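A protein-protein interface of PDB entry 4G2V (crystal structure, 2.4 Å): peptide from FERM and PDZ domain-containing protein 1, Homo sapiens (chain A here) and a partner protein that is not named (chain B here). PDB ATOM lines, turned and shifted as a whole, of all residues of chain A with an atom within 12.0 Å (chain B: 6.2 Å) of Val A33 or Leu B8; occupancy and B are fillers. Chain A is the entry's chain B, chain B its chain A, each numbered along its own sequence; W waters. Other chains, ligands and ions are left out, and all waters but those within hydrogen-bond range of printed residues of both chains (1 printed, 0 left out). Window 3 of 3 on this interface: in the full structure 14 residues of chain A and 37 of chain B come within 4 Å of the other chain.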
ATOM      1  N   GLU A  29      22.387  -2.322  12.711  1.00  0.00           N
ATOM      2  CA  GLU A  29      22.297  -3.482  13.578  1.00  0.00           C
ATOM      3  C   GLU A  29      20.849  -3.944  13.622  1.00  0.00           C
ATOM      4  O   GLU A  29      19.926  -3.129  13.664  1.00  0.00           O
ATOM      5  CB  GLU A  29      22.820  -3.160  14.977  1.00  0.00           C
ATOM      6  CG  GLU A  29      24.287  -2.758  14.986  1.00  0.00           C
ATOM      7  CD  GLU A  29      25.179  -3.834  14.395  1.00  0.00           C
ATOM      8  OE1 GLU A  29      25.125  -4.979  14.886  1.00  0.00           O
ATOM      9  OE2 GLU A  29      25.925  -3.540  13.437  1.00  0.00           O
ATOM     10  N   THR A  30      20.652  -5.255  13.591  1.00  0.00           N
ATOM     11  CA  THR A  30      19.308  -5.803  13.517  1.00  0.00           C
ATOM     12  C   THR A  30      18.946  -6.622  14.748  1.00  0.00           C
ATOM     13  O   THR A  30      19.801  -7.254  15.377  1.00  0.00           O
ATOM     14  CB  THR A  30      19.123  -6.656  12.252  1.00  0.00           C
ATOM     15  OG1 THR A  30      20.082  -7.718  12.250  1.00  0.00           O
ATOM     16  CG2 THR A  30      19.330  -5.803  11.010  1.00  0.00           C
ATOM     17  N   LYS A  31      17.667  -6.581  15.095  1.00  0.00           N
ATOM     18  CA  LYS A  31      17.132  -7.398  16.173  1.00  0.00           C
ATOM     19  C   LYS A  31      15.959  -8.229  15.645  1.00  0.00           C
ATOM     20  O   LYS A  31      15.343  -7.879  14.638  1.00  0.00           O
ATOM     21  CB  LYS A  31      16.688  -6.511  17.343  1.00  0.00           C
ATOM     22  CG  LYS A  31      17.816  -5.688  17.979  1.00  0.00           C
ATOM     23  CD  LYS A  31      17.301  -4.769  19.095  1.00  0.00           C
ATOM     24  CE  LYS A  31      18.399  -3.832  19.598  1.00  0.00           C
ATOM     25  NZ  LYS A  31      18.071  -3.174  20.894  1.00  0.00           N
ATOM     26  N   SER A  32      15.661  -9.336  16.311  1.00  0.00           N
ATOM     27  CA  SER A  32      14.506 -10.141  15.942  1.00  0.00           C
ATOM     28  C   SER A  32      13.661 -10.439  17.173  1.00  0.00           C
ATOM     29  O   SER A  32      14.161 -10.403  18.297  1.00  0.00           O
ATOM     30  CB  SER A  32      14.955 -11.444  15.264  1.00  0.00           C
ATOM     31  OG  SER A  32      13.844 -12.233  14.859  1.00  0.00           O
ATOM     32  N   VAL A  33      12.383 -10.733  16.961  1.00  0.00           N
ATOM     33  CA  VAL A  33      11.506 -11.141  18.054  1.00  0.00           C
ATOM     34  C   VAL A  33      11.715 -12.615  18.400  1.00  0.00           C
ATOM     35  O   VAL A  33      11.274 -13.080  19.450  1.00  0.00           O
ATOM     36  CB  VAL A  33      10.019 -10.892  17.727  1.00  0.00           C
ATOM     37  CG1 VAL A  33       9.791  -9.425  17.392  1.00  0.00           C
ATOM     38  CG2 VAL A  33       9.562 -11.785  16.583  1.00  0.00           C
ATOM     39  N   ILE A  34      12.386 -13.341  17.507  1.00  0.00           N
ATOM     40  CA  ILE A  34      12.743 -14.740  17.744  1.00  0.00           C
ATOM     41  C   ILE A  34      14.256 -14.945  17.675  1.00  0.00           C
ATOM     42  O   ILE A  34      14.924 -14.386  16.806  1.00  0.00           O
ATOM     43  CB  ILE A  34      12.054 -15.698  16.736  1.00  0.00           C
ATOM     44  CG1 ILE A  34      12.269 -15.228  15.293  1.00  0.00           C
ATOM     45  CG2 ILE A  34      10.567 -15.818  17.035  1.00  0.00           C
ATOM     46  CD1 ILE A  34      13.469 -15.850  14.605  1.00  0.00           C
ATOM     47  N   ASP A  35      14.792 -15.733  18.601  1.00  0.00           N
ATOM     48  CA  ASP A  35      16.203 -16.116  18.561  1.00  0.00           C
ATOM     49  C   ASP A  35      16.348 -17.624  18.352  1.00  0.00           C
ATOM     50  O   ASP A  35      16.007 -18.416  19.233  1.00  0.00           O
ATOM     51  CB  ASP A  35      16.924 -15.676  19.839  1.00  0.00           C
ATOM     52  CG  ASP A  35      18.384 -16.103  19.866  1.00  0.00           C
ATOM     53  OD1 ASP A  35      19.232 -15.370  19.313  1.00  0.00           O
ATOM     54  OD2 ASP A  35      18.687 -17.168  20.445  1.00  0.00           O
ATOM     55  N   SER A  36      16.851 -18.015  17.184  1.00  0.00           N
ATOM     56  CA  SER A  36      17.018 -19.428  16.847  1.00  0.00           C
ATOM     57  C   SER A  36      17.945 -20.131  17.833  1.00  0.00           C
ATOM     58  O   SER A  36      17.489 -20.765  18.785  1.00  0.00           O
ATOM     59  CB  SER A  36      17.543 -19.577  15.423  1.00  0.00           C
ATOM     60  N   GLY B   3      -2.496  -9.952  24.683  1.00  0.00           N
ATOM     61  CA  GLY B   3      -2.175  -9.515  23.338  1.00  0.00           C
ATOM     62  C   GLY B   3      -0.710  -9.693  22.984  1.00  0.00           C
ATOM     63  O   GLY B   3      -0.212  -9.080  22.041  1.00  0.00           O
ATOM     64  N   SER B   4      -0.015 -10.538  23.742  1.00  0.00           N
ATOM     65  CA  SER B   4       1.406 -10.786  23.511  1.00  0.00           C
ATOM     66  C   SER B   4       1.663 -11.697  22.308  1.00  0.00           C
ATOM     67  O   SER B   4       2.540 -11.416  21.487  1.00  0.00           O
ATOM     68  CB  SER B   4       2.061 -11.365  24.767  1.00  0.00           C
ATOM     69  OG  SER B   4       2.028 -10.428  25.833  1.00  0.00           O
ATOM     70  N   ALA B   5       0.904 -12.787  22.210  1.00  0.00           N
ATOM     71  CA  ALA B   5       1.057 -13.731  21.105  1.00  0.00           C
ATOM     72  C   ALA B   5       0.688 -13.068  19.785  1.00  0.00           C
ATOM     73  O   ALA B   5       1.396 -13.209  18.787  1.00  0.00           O
ATOM     74  CB  ALA B   5       0.200 -14.966  21.338  1.00  0.00           C
ATOM     75  N   SER B   6      -0.427 -12.342  19.795  1.00  0.00           N
ATOM     76  CA  SER B   6      -0.865 -11.563  18.644  1.00  0.00           C
ATOM     77  C   SER B   6       0.221 -10.570  18.231  1.00  0.00           C
ATOM     78  O   SER B   6       0.465 -10.355  17.043  1.00  0.00           O
ATOM     79  CB  SER B   6      -2.153 -10.810  18.984  1.00  0.00           C
ATOM     80  OG  SER B   6      -2.937 -11.538  19.914  1.00  0.00           O
ATOM     81  N   CYS B   7       0.865  -9.966  19.223  1.00  0.00           N
ATOM     82  CA  CYS B   7       1.967  -9.046  18.975  1.00  0.00           C
ATOM     83  C   CYS B   7       3.140  -9.792  18.353  1.00  0.00           C
ATOM     84  O   CYS B   7       3.668  -9.392  17.316  1.00  0.00           O
ATOM     85  CB  CYS B   7       2.400  -8.371  20.278  1.00  0.00           C
ATOM     86  SG  CYS B   7       3.855  -7.312  20.122  1.00  0.00           S
ATOM     87  N   LEU B   8       3.540 -10.882  18.996  1.00  0.00           N
ATOM     88  CA  LEU B   8       4.575 -11.753  18.457  1.00  0.00           C
ATOM     89  C   LEU B   8       4.263 -12.117  17.003  1.00  0.00           C
ATOM     90  O   LEU B   8       5.116 -11.989  16.125  1.00  0.00           O
ATOM     91  CB  LEU B   8       4.685 -13.017  19.307  1.00  0.00           C
ATOM     92  CG  LEU B   8       6.069 -13.650  19.426  1.00  0.00           C
ATOM     93  CD1 LEU B   8       7.127 -12.589  19.694  1.00  0.00           C
ATOM     94  CD2 LEU B   8       6.072 -14.708  20.520  1.00  0.00           C
ATOM     95  N   GLU B   9       3.030 -12.553  16.756  1.00  0.00           N
ATOM     96  CA  GLU B   9       2.610 -12.966  15.418  1.00  0.00           C
ATOM     97  C   GLU B   9       2.681 -11.835  14.390  1.00  0.00           C
ATOM     98  O   GLU B   9       3.239 -12.006  13.305  1.00  0.00           O
ATOM     99  CB  GLU B   9       1.199 -13.572  15.450  1.00  0.00           C
ATOM    100  CG  GLU B   9       1.098 -14.885  16.226  1.00  0.00           C
ATOM    101  CD  GLU B   9      -0.236 -15.591  16.025  1.00  0.00           C
ATOM    102  OE1 GLU B   9      -0.351 -16.398  15.074  1.00  0.00           O
ATOM    103  OE2 GLU B   9      -1.167 -15.343  16.821  1.00  0.00           O
ATOM    104  N   LEU B  10       2.113 -10.682  14.732  1.00  0.00           N
ATOM    105  CA  LEU B  10       2.130  -9.530  13.835  1.00  0.00           C
ATOM    106  C   LEU B  10       3.556  -9.097  13.495  1.00  0.00           C
ATOM    107  O   LEU B  10       3.846  -8.721  12.359  1.00  0.00           O
ATOM    108  CB  LEU B  10       1.348  -8.358  14.437  1.00  0.00           C
ATOM    109  CG  LEU B  10      -0.175  -8.500  14.508  1.00  0.00           C
ATOM    110  CD1 LEU B  10      -0.784  -7.315  15.245  1.00  0.00           C
ATOM    111  CD2 LEU B  10      -0.779  -8.639  13.117  1.00  0.00           C
ATOM    112  N   ALA B  11       4.444  -9.150  14.480  1.00  0.00           N
ATOM    113  CA  ALA B  11       5.830  -8.751  14.258  1.00  0.00           C
ATOM    114  C   ALA B  11       6.535  -9.728  13.312  1.00  0.00           C
ATOM    115  O   ALA B  11       7.375  -9.329  12.502  1.00  0.00           O
ATOM    116  CB  ALA B  11       6.575  -8.635  15.583  1.00  0.00           C
ATOM    117  N   LEU B  12       6.176 -11.004  13.408  1.00  0.00           N
ATOM    118  CA  LEU B  12       6.715 -12.013  12.505  1.00  0.00           C
ATOM    119  C   LEU B  12       6.381 -11.712  11.048  1.00  0.00           C
ATOM    120  O   LEU B  12       7.209 -11.929  10.162  1.00  0.00           O
ATOM    121  CB  LEU B  12       6.204 -13.401  12.878  1.00  0.00           C
ATOM    122  CG  LEU B  12       6.974 -14.110  13.989  1.00  0.00           C
ATOM    123  CD1 LEU B  12       6.321 -15.444  14.302  1.00  0.00           C
ATOM    124  CD2 LEU B  12       8.431 -14.303  13.585  1.00  0.00           C
ATOM    125  N   GLU B  13       5.168 -11.223  10.799  1.00  0.00           N
ATOM    126  CA  GLU B  13       4.779 -10.841   9.445  1.00  0.00           C
ATOM    127  C   GLU B  13       5.645  -9.693   8.956  1.00  0.00           C
ATOM    128  O   GLU B  13       6.135  -9.710   7.824  1.00  0.00           O
ATOM    129  CB  GLU B  13       3.300 -10.459   9.373  1.00  0.00           C
ATOM    130  CG  GLU B  13       2.403 -11.574   8.873  1.00  0.00           C
ATOM    131  CD  GLU B  13       3.019 -12.324   7.706  1.00  0.00           C
ATOM    132  OE1 GLU B  13       3.726 -13.331   7.950  1.00  0.00           O
ATOM    133  OE2 GLU B  13       2.796 -11.902   6.549  1.00  0.00           O
ATOM    134  N   GLU B  15       8.667  -8.771  10.027  1.00  0.00           N
ATOM    135  CA  GLU B  15      10.022  -9.265   9.791  1.00  0.00           C
ATOM    136  C   GLU B  15      10.123  -9.945   8.437  1.00  0.00           C
ATOM    137  O   GLU B  15      11.074  -9.730   7.688  1.00  0.00           O
ATOM    138  CB  GLU B  15      10.441 -10.253  10.880  1.00  0.00           C
ATOM    139  CG  GLU B  15      10.492  -9.645  12.261  1.00  0.00           C
ATOM    140  CD  GLU B  15      11.398 -10.407  13.201  1.00  0.00           C
ATOM    141  OE1 GLU B  15      11.347 -10.127  14.418  1.00  0.00           O
ATOM    142  OE2 GLU B  15      12.166 -11.272  12.722  1.00  0.00           O
ATOM    143  N   PHE B  30       4.443  -4.100  11.891  1.00  0.00           N
ATOM    144  CA  PHE B  30       5.149  -3.721  13.114  1.00  0.00           C
ATOM    145  C   PHE B  30       4.330  -2.707  13.904  1.00  0.00           C
ATOM    146  O   PHE B  30       4.213  -2.807  15.126  1.00  0.00           O
ATOM    147  CB  PHE B  30       6.528  -3.142  12.801  1.00  0.00           C
ATOM    148  CG  PHE B  30       7.545  -4.176  12.443  1.00  0.00           C
ATOM    149  CD1 PHE B  30       7.670  -5.332  13.197  1.00  0.00           C
ATOM    150  CD2 PHE B  30       8.373  -4.003  11.346  1.00  0.00           C
ATOM    151  CE1 PHE B  30       8.608  -6.294  12.868  1.00  0.00           C
ATOM    152  CE2 PHE B  30       9.309  -4.964  11.011  1.00  0.00           C
ATOM    153  CZ  PHE B  30       9.426  -6.108  11.775  1.00  0.00           C
ATOM    154  N   ALA B  33       1.672  -4.467  15.556  1.00  0.00           N
ATOM    155  CA  ALA B  33       2.191  -5.168  16.721  1.00  0.00           C
ATOM    156  C   ALA B  33       2.319  -4.207  17.896  1.00  0.00           C
ATOM    157  O   ALA B  33       1.922  -4.529  19.014  1.00  0.00           O
ATOM    158  CB  ALA B  33       3.533  -5.811  16.398  1.00  0.00           C
ATOM    159  N   THR B  38       2.645  -5.562  24.235  1.00  0.00           N
ATOM    160  CA  THR B  38       3.116  -6.761  24.921  1.00  0.00           C
ATOM    161  C   THR B  38       3.741  -6.411  26.262  1.00  0.00           C
ATOM    162  O   THR B  38       4.190  -5.287  26.474  1.00  0.00           O
ATOM    163  CB  THR B  38       4.182  -7.506  24.100  1.00  0.00           C
ATOM    164  OG1 THR B  38       4.775  -8.530  24.911  1.00  0.00           O
ATOM    165  CG2 THR B  38       5.277  -6.542  23.653  1.00  0.00           C
ATOM    166  N   LYS B  42      11.703  -6.704  25.759  1.00  0.00           N
ATOM    167  CA  LYS B  42      12.748  -7.047  24.802  1.00  0.00           C
ATOM    168  C   LYS B  42      12.147  -7.278  23.418  1.00  0.00           C
ATOM    169  O   LYS B  42      12.799  -7.041  22.402  1.00  0.00           O
ATOM    170  CB  LYS B  42      13.549  -8.266  25.270  1.00  0.00           C
ATOM    171  CG  LYS B  42      14.911  -8.387  24.605  1.00  0.00           C
ATOM    172  CD  LYS B  42      15.930  -9.051  25.518  1.00  0.00           C
ATOM    173  CE  LYS B  42      17.321  -9.010  24.898  1.00  0.00           C
ATOM    174  NZ  LYS B  42      18.361  -9.586  25.797  1.00  0.00           N
ATOM    175  N   THR B  43      10.896  -7.728  23.386  1.00  0.00           N
ATOM    176  CA  THR B  43      10.179  -7.907  22.127  1.00  0.00           C
ATOM    177  C   THR B  43       9.829  -6.555  21.519  1.00  0.00           C
ATOM    178  O   THR B  43      10.005  -6.344  20.320  1.00  0.00           O
ATOM    179  CB  THR B  43       8.895  -8.744  22.310  1.00  0.00           C
ATOM    180  OG1 THR B  43       9.241 -10.048  22.788  1.00  0.00           O
ATOM    181  CG2 THR B  43       8.147  -8.880  20.989  1.00  0.00           C
ATOM    182  N   ALA B  46      12.937  -5.052  20.020  1.00  0.00           N
ATOM    183  CA  ALA B  46      13.204  -5.609  18.698  1.00  0.00           C
ATOM    184  C   ALA B  46      12.292  -4.972  17.662  1.00  0.00           C
ATOM    185  O   ALA B  46      12.718  -4.639  16.556  1.00  0.00           O
ATOM    186  CB  ALA B  46      13.029  -7.134  18.706  1.00  0.00           C
ATOM    187  N   ILE B  47      11.030  -4.802  18.032  1.00  0.00           N
ATOM    188  CA  ILE B  47      10.055  -4.180  17.151  1.00  0.00           C
ATOM    189  C   ILE B  47      10.422  -2.733  16.828  1.00  0.00           C
ATOM    190  O   ILE B  47      10.432  -2.336  15.662  1.00  0.00           O
ATOM    191  CB  ILE B  47       8.643  -4.262  17.752  1.00  0.00           C
ATOM    192  CG1 ILE B  47       8.211  -5.729  17.850  1.00  0.00           C
ATOM    193  CG2 ILE B  47       7.659  -3.465  16.912  1.00  0.00           C
ATOM    194  CD1 ILE B  47       6.866  -5.938  18.512  1.00  0.00           C
ATOM    195  N   GLN B  50      13.389  -2.592  14.450  1.00  0.00           N
ATOM    196  CA  GLN B  50      13.070  -2.933  13.065  1.00  0.00           C
ATOM    197  C   GLN B  50      12.216  -1.869  12.380  1.00  0.00           C
ATOM    198  O   GLN B  50      12.368  -1.622  11.184  1.00  0.00           O
ATOM    199  CB  GLN B  50      12.432  -4.320  12.976  1.00  0.00           C
ATOM    200  CG  GLN B  50      13.436  -5.432  13.245  1.00  0.00           C
ATOM    201  CD  GLN B  50      12.797  -6.799  13.335  1.00  0.00           C
ATOM    202  OE1 GLN B  50      12.798  -7.563  12.369  1.00  0.00           O
ATOM    203  NE2 GLN B  50      12.255  -7.124  14.505  1.00  0.00           N
HETATM  204  O   HOH W   1      11.590 -11.223  21.689  1.00  0.00           O
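The side-chain carboxylate (OE2) of Glu B15 sits at hydrogen-bond distance from the side-chain hydroxyl (OG) of Ser A32, at 2.9 Å. OE1 of Glu B15 sits at hydrogen-bond distance from N of Val A33. The side-chain amide nitrogen of Gln B50 lies close to the backbone carbonyl oxygen of Lys A31 (3.2 Å).
Among the printed residues, merely in contact across the chains: Ser A32 with Ala B46, Val A33 with Ala B11, Lys A31 with Ala B46, Val A33 with Leu B8 and Val A33 with Thr B43.
Of the 8 printed residues of chain A, 3 touch a printed residue of chain B. Printed residues of chain A that touch a printed residue of chain B: Lys A31, Ser A32 and Val A33. Of the 20 printed residues of chain B, 6 touch a printed residue of chain A. Hydrophobic or aromatic side chains of chain B within 4 Å of the printed part of chain A: Leu B8, Ala B11 and Ala B46. Among the printed residues, 8 pairs touch across the chains.
Water W1 bridges the side-chain hydroxyl (OG1) of Thr B43 (2.8 Å) and the backbone carbonyl oxygen (O) of Val A33 (2.9 Å).
The side-chain carboxylate (OE1) of Glu B15 sits at hydrogen-bond distance from the side-chain amide nitrogen (NE2) of Gln B50 (3.1 Å). NE2 of Gln B50 lies within hydrogen-bond range of O of Ala B46, at 3.3 Å. OG of Ser A32 is in hydrogen-bond range of O of Ile A34.
Printed residues of chain B within 4 Å of Val A33: Leu B8 (3.9 Å), Ala B11 (3.8 Å), Glu B15 (2.8 Å) and Thr B43 (3.99 Å). Leu B8 touches just one residue of chain A: Val A33 (3.9 Å). No residue of chain A comes within 4 Å of Ser B4. No residue of chain A comes within 4 Å of Ala B5. No residue of chain A comes within 4 Å of Cys B7. No residue of chain A comes within 4 Å of Glu B9. No residue of chain A comes within 4 Å of Leu B10. Of chain A, only Val A33 (3.8 Å) comes within 4 Å of Ala B11. No residue of chain A comes within 4 Å of Leu B12. No residue of chain A comes within 4 Å of Ala B33. Ala B46 touches just these residues of chain A: Lys A31 and Ser A32. Printed residues of chain A within 4 Å of Glu B15: Ser A32 (2.9 Å) and Val A33 (2.8 Å). Of the printed residues of chain B, Ser A32 touches Glu B15 and Ala B46. Of the printed residues of chain A, Thr B43 touches Val A33. Of the printed residues of chain A, Gln B50 touches Lys A31 (3.1 Å). Printed residues of chain B within 4 Å of Lys A31: Ala B46 and Gln B50. Glu B13 touches none of the printed residues of chain A. Asp A35 touches none of the printed residues of chain B.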
